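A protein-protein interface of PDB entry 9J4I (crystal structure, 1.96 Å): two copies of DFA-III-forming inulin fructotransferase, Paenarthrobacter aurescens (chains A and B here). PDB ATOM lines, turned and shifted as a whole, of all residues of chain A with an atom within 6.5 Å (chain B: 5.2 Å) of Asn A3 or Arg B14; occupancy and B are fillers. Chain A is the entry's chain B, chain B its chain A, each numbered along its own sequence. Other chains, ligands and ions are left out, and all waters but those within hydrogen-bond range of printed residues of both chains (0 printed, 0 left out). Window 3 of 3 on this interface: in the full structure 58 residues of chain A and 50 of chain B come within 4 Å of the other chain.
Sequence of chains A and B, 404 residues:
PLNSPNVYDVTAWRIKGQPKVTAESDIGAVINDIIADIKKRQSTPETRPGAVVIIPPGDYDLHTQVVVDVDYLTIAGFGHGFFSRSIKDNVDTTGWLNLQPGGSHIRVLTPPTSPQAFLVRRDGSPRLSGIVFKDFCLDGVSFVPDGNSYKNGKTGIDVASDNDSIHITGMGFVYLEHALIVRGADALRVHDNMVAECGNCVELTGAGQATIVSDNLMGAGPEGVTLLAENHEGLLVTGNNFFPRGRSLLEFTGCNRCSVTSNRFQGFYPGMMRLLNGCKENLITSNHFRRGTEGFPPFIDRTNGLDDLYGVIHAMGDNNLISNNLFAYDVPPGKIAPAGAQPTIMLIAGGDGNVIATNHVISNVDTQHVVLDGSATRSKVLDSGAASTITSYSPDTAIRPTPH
Among the printed residues, pairs that only touch across the chains: Leu A2 with Asp B9, Ser A4 with Thr B11, Asn A3 with Ala B12 and Asn A3 with Arg B14.
The guanidinium group (NH2) of Arg B14 sits at hydrogen-bond distance from the backbone carbonyl oxygen (O) of Thr B11 (2.8 Å).
The side-chain carboxylate (OD1) of Asp B9 is in hydrogen-bond range of the side-chain hydroxyl (OG1) of Thr B11, at 2.6 Å.
No position is printed for both chains.
Of the 6 pairs that touch across the chains among the printed residues, none has its exchanged pair printed and touching as well.
The backbone carbonyl oxygen (O) of Thr B11 is in hydrogen-bond range of the side-chain amide nitrogen (ND2) of Asn A3 (3.0 Å).
OD2 of Asp B9 lies within hydrogen-bond range of N of Asn A3.
Of chain B, only Asp B9, Thr B11, Ala B12 and Arg B14 come within 4 Å of Asn A3.
Of the printed residues of chain A, Ala B12 touches Asn A3.
Of the printed residues of chain A, Asp B9 touches Leu A2 (3.5 Å) and Asn A3 (2.8 Å).
Printed residues of chain A within 4 Å of Thr B11: Asn A3 (3.0 Å) and Ser A4 (3.6 Å).
Printed residues of chain A that touch a printed residue of chain B: Leu A2, Asn A3 and Ser A4.
Hydrophobic or aromatic side chains of chain A within 4 Å of the printed part of chain B: Leu A2.
Among the printed residues, no Asp or Glu carboxylate lies within 4 Å of a Lys or Arg side-chain nitrogen of the other chain.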
ATOM      1  N   PRO A   1      -0.669 -16.410  -4.620  1.00  0.00           N
ATOM      2  CA  PRO A   1       0.449 -15.890  -5.436  1.00  0.00           C
ATOM      3  C   PRO A   1       0.112 -15.945  -6.938  1.00  0.00           C
ATOM      4  O   PRO A   1       0.070 -14.917  -7.580  1.00  0.00           O
ATOM      5  CB  PRO A   1       1.664 -16.773  -5.094  1.00  0.00           C
ATOM      6  CG  PRO A   1       1.075 -17.987  -4.399  1.00  0.00           C
ATOM      7  CD  PRO A   1      -0.201 -17.492  -3.744  1.00  0.00           C
ATOM      8  N   LEU A   2      -0.097 -17.152  -7.468  1.00  0.00           N
ATOM      9  CA  LEU A   2      -0.723 -17.408  -8.791  1.00  0.00           C
ATOM     10  C   LEU A   2      -2.097 -18.040  -8.526  1.00  0.00           C
ATOM     11  O   LEU A   2      -2.321 -18.462  -7.386  1.00  0.00           O
ATOM     12  CB  LEU A   2       0.202 -18.315  -9.612  1.00  0.00           C
ATOM     13  CG  LEU A   2       1.487 -17.641 -10.104  1.00  0.00           C
ATOM     14  CD1 LEU A   2       2.507 -18.650 -10.582  1.00  0.00           C
ATOM     15  CD2 LEU A   2       1.192 -16.640 -11.215  1.00  0.00           C
ATOM     16  N   ASN A   3      -3.000 -18.075  -9.503  1.00  0.00           N
ATOM     17  CA  ASN A   3      -4.385 -18.570  -9.269  1.00  0.00           C
ATOM     18  C   ASN A   3      -4.433 -20.097  -9.394  1.00  0.00           C
ATOM     19  O   ASN A   3      -5.424 -20.610  -9.948  1.00  0.00           O
ATOM     20  CB  ASN A   3      -5.405 -17.930 -10.212  1.00  0.00           C
ATOM     21  CG  ASN A   3      -6.818 -18.064  -9.684  1.00  0.00           C
ATOM     22  OD1 ASN A   3      -7.037 -17.998  -8.476  1.00  0.00           O
ATOM     23  ND2 ASN A   3      -7.779 -18.247 -10.572  1.00  0.00           N
ATOM     24  N   SER A   4      -3.387 -20.796  -8.941  1.00  0.00           N
ATOM     25  CA  SER A   4      -3.278 -22.277  -8.957  1.00  0.00           C
ATOM     26  C   SER A   4      -2.982 -22.747  -7.545  1.00  0.00           C
ATOM     27  O   SER A   4      -2.088 -22.216  -6.897  1.00  0.00           O
ATOM     28  CB  SER A   4      -2.207 -22.759  -9.898  1.00  0.00           C
ATOM     29  OG  SER A   4      -1.913 -24.134  -9.672  1.00  0.00           O
ATOM     30  N   PRO A   5      -3.653 -23.811  -7.066  1.00  0.00           N
ATOM     31  CA  PRO A   5      -3.317 -24.384  -5.764  1.00  0.00           C
ATOM     32  C   PRO A   5      -1.974 -25.136  -5.771  1.00  0.00           C
ATOM     33  O   PRO A   5      -1.576 -25.576  -4.721  1.00  0.00           O
ATOM     34  CB  PRO A   5      -4.481 -25.344  -5.486  1.00  0.00           C
ATOM     35  CG  PRO A   5      -5.004 -25.720  -6.870  1.00  0.00           C
ATOM     36  CD  PRO A   5      -4.751 -24.516  -7.752  1.00  0.00           C
ATOM     37  N   VAL A   7       0.940 -23.854  -6.612  1.00  0.00           N
ATOM     38  CA  VAL A   7       2.051 -22.874  -6.447  1.00  0.00           C
ATOM     39  C   VAL A   7       2.094 -22.466  -4.981  1.00  0.00           C
ATOM     40  O   VAL A   7       1.101 -21.924  -4.478  1.00  0.00           O
ATOM     41  CB  VAL A   7       1.923 -21.652  -7.369  1.00  0.00           C
ATOM     42  CG1 VAL A   7       3.051 -20.664  -7.120  1.00  0.00           C
ATOM     43  CG2 VAL A   7       1.881 -22.080  -8.823  1.00  0.00           C
ATOM     44  N   ASP B   9      -0.980 -15.043 -16.099  1.00  0.00           N
ATOM     45  CA  ASP B   9      -1.110 -16.353 -15.432  1.00  0.00           C
ATOM     46  C   ASP B   9      -2.280 -17.046 -16.135  1.00  0.00           C
ATOM     47  O   ASP B   9      -3.387 -16.499 -16.056  1.00  0.00           O
ATOM     48  CB  ASP B   9      -1.270 -16.119 -13.928  1.00  0.00           C
ATOM     49  CG  ASP B   9      -1.816 -17.310 -13.167  1.00  0.00           C
ATOM     50  OD1 ASP B   9      -1.838 -18.422 -13.741  1.00  0.00           O
ATOM     51  OD2 ASP B   9      -2.219 -17.108 -12.009  1.00  0.00           O
ATOM     52  N   VAL B  10      -2.047 -18.168 -16.824  1.00  0.00           N
ATOM     53  CA  VAL B  10      -3.104 -18.874 -17.615  1.00  0.00           C
ATOM     54  C   VAL B  10      -4.240 -19.316 -16.694  1.00  0.00           C
ATOM     55  O   VAL B  10      -5.360 -19.466 -17.218  1.00  0.00           O
ATOM     56  CB  VAL B  10      -2.610 -20.085 -18.435  1.00  0.00           C
ATOM     57  CG1 VAL B  10      -1.621 -19.689 -19.509  1.00  0.00           C
ATOM     58  CG2 VAL B  10      -2.098 -21.240 -17.575  1.00  0.00           C
ATOM     59  N   THR B  11      -3.974 -19.543 -15.401  1.00  0.00           N
ATOM     60  CA  THR B  11      -5.014 -19.985 -14.429  1.00  0.00           C
ATOM     61  C   THR B  11      -5.830 -18.786 -13.937  1.00  0.00           C
ATOM     62  O   THR B  11      -6.885 -19.019 -13.364  1.00  0.00           O
ATOM     63  CB  THR B  11      -4.423 -20.776 -13.253  1.00  0.00           C
ATOM     64  OG1 THR B  11      -3.561 -19.947 -12.475  1.00  0.00           O
ATOM     65  CG2 THR B  11      -3.668 -22.003 -13.719  1.00  0.00           C
ATOM     66  N   ALA B  12      -5.363 -17.560 -14.155  1.00  0.00           N
ATOM     67  CA  ALA B  12      -6.027 -16.322 -13.686  1.00  0.00           C
ATOM     68  C   ALA B  12      -6.748 -15.642 -14.850  1.00  0.00           C
ATOM     69  O   ALA B  12      -7.710 -14.912 -14.589  1.00  0.00           O
ATOM     70  CB  ALA B  12      -5.021 -15.384 -13.075  1.00  0.00           C
ATOM     71  N   TRP B  13      -6.253 -15.820 -16.076  1.00  0.00           N
ATOM     72  CA  TRP B  13      -6.810 -15.165 -17.281  1.00  0.00           C
ATOM     73  C   TRP B  13      -8.203 -15.727 -17.558  1.00  0.00           C
ATOM     74  O   TRP B  13      -8.341 -16.955 -17.659  1.00  0.00           O
ATOM     75  CB  TRP B  13      -5.900 -15.315 -18.501  1.00  0.00           C
ATOM     76  CG  TRP B  13      -6.424 -14.521 -19.654  1.00  0.00           C
ATOM     77  CD1 TRP B  13      -7.158 -14.985 -20.704  1.00  0.00           C
ATOM     78  CD2 TRP B  13      -6.287 -13.103 -19.849  1.00  0.00           C
ATOM     79  NE1 TRP B  13      -7.474 -13.957 -21.538  1.00  0.00           N
ATOM     80  CE2 TRP B  13      -6.957 -12.791 -21.046  1.00  0.00           C
ATOM     81  CE3 TRP B  13      -5.679 -12.069 -19.124  1.00  0.00           C
ATOM     82  CZ2 TRP B  13      -7.030 -11.489 -21.542  1.00  0.00           C
ATOM     83  CZ3 TRP B  13      -5.762 -10.783 -19.609  1.00  0.00           C
ATOM     84  CH2 TRP B  13      -6.418 -10.502 -20.809  1.00  0.00           C
ATOM     85  N   ARG B  14      -9.193 -14.845 -17.661  1.00  0.00           N
ATOM     86  CA  ARG B  14     -10.577 -15.224 -18.029  1.00  0.00           C
ATOM     87  C   ARG B  14     -10.861 -14.621 -19.403  1.00  0.00           C
ATOM     88  O   ARG B  14     -10.485 -13.466 -19.631  1.00  0.00           O
ATOM     89  CB  ARG B  14     -11.542 -14.809 -16.911  1.00  0.00           C
ATOM     90  CG  ARG B  14     -11.433 -15.675 -15.658  1.00  0.00           C
ATOM     91  CD  ARG B  14     -11.571 -17.171 -15.931  1.00  0.00           C
ATOM     92  NE  ARG B  14     -11.562 -17.993 -14.722  1.00  0.00           N
ATOM     93  CZ  ARG B  14     -10.478 -18.517 -14.138  1.00  0.00           C
ATOM     94  NH1 ARG B  14     -10.613 -19.239 -13.037  1.00  0.00           N
ATOM     95  NH2 ARG B  14      -9.268 -18.323 -14.639  1.00  0.00           N
ATOM     96  N   ILE B  15     -11.440 -15.408 -20.301  1.00  0.00           N
ATOM     97  CA  ILE B  15     -11.880 -14.919 -21.632  1.00  0.00           C
ATOM     98  C   ILE B  15     -13.227 -14.226 -21.425  1.00  0.00           C
ATOM     99  O   ILE B  15     -14.189 -14.893 -20.986  1.00  0.00           O
ATOM    100  CB  ILE B  15     -11.955 -16.057 -22.654  1.00  0.00           C
ATOM    101  CG1 ILE B  15     -10.652 -16.863 -22.728  1.00  0.00           C
ATOM    102  CG2 ILE B  15     -12.351 -15.490 -24.011  1.00  0.00           C
ATOM    103  CD1 ILE B  15     -10.683 -18.025 -23.726  1.00  0.00           C
ATOM    104  N   LYS B  16     -13.285 -12.929 -21.684  1.00  0.00           N
ATOM    105  CA  LYS B  16     -14.536 -12.155 -21.491  1.00  0.00           C
ATOM    106  C   LYS B  16     -15.603 -12.763 -22.408  1.00  0.00           C
ATOM    107  O   LYS B  16     -15.326 -12.977 -23.596  1.00  0.00           O
ATOM    108  CB  LYS B  16     -14.301 -10.664 -21.731  1.00  0.00           C
ATOM    109  CG  LYS B  16     -15.348  -9.771 -21.075  1.00  0.00           C
ATOM    110  CD  LYS B  16     -15.352  -8.355 -21.597  1.00  0.00           C
ATOM    111  CE  LYS B  16     -16.587  -7.586 -21.176  1.00  0.00           C
ATOM    112  NZ  LYS B  16     -16.657  -6.277 -21.863  1.00  0.00           N
ATOM    113  N   PRO B  19     -16.720 -17.848 -19.872  1.00  0.00           N
ATOM    114  CA  PRO B  19     -16.253 -18.271 -18.550  1.00  0.00           C
ATOM    115  C   PRO B  19     -15.980 -19.782 -18.423  1.00  0.00           C
ATOM    116  O   PRO B  19     -15.251 -20.128 -17.523  1.00  0.00           O
ATOM    117  CB  PRO B  19     -17.380 -17.837 -17.597  1.00  0.00           C
ATOM    118  CG  PRO B  19     -18.610 -17.733 -18.485  1.00  0.00           C
ATOM    119  CD  PRO B  19     -18.099 -17.339 -19.855  1.00  0.00           C
ATOM    120  N   THR B  22     -11.306 -22.455 -19.759  1.00  0.00           N
ATOM    121  CA  THR B  22     -10.246 -22.271 -18.740  1.00  0.00           C
ATOM    122  C   THR B  22      -8.958 -22.903 -19.263  1.00  0.00           C
ATOM    123  O   THR B  22      -9.022 -23.612 -20.272  1.00  0.00           O
ATOM    124  CB  THR B  22     -10.645 -22.931 -17.413  1.00  0.00           C
ATOM    125  OG1 THR B  22     -10.810 -24.316 -17.716  1.00  0.00           O
ATOM    126  CG2 THR B  22     -11.910 -22.353 -16.815  1.00  0.00           C
ATOM    127  N   ASP B  33      -6.308 -15.949 -26.619  1.00  0.00           N
ATOM    128  CA  ASP B  33      -6.982 -14.742 -26.070  1.00  0.00           C
ATOM    129  C   ASP B  33      -5.945 -13.806 -25.452  1.00  0.00           C
ATOM    130  O   ASP B  33      -6.048 -12.574 -25.646  1.00  0.00           O
ATOM    131  CB  ASP B  33      -8.070 -15.113 -25.064  1.00  0.00           C
ATOM    132  CG  ASP B  33      -9.059 -13.978 -24.900  1.00  0.00           C
ATOM    133  OD1 ASP B  33      -9.670 -13.608 -25.914  1.00  0.00           O
ATOM    134  OD2 ASP B  33      -9.185 -13.458 -23.775  1.00  0.00           O
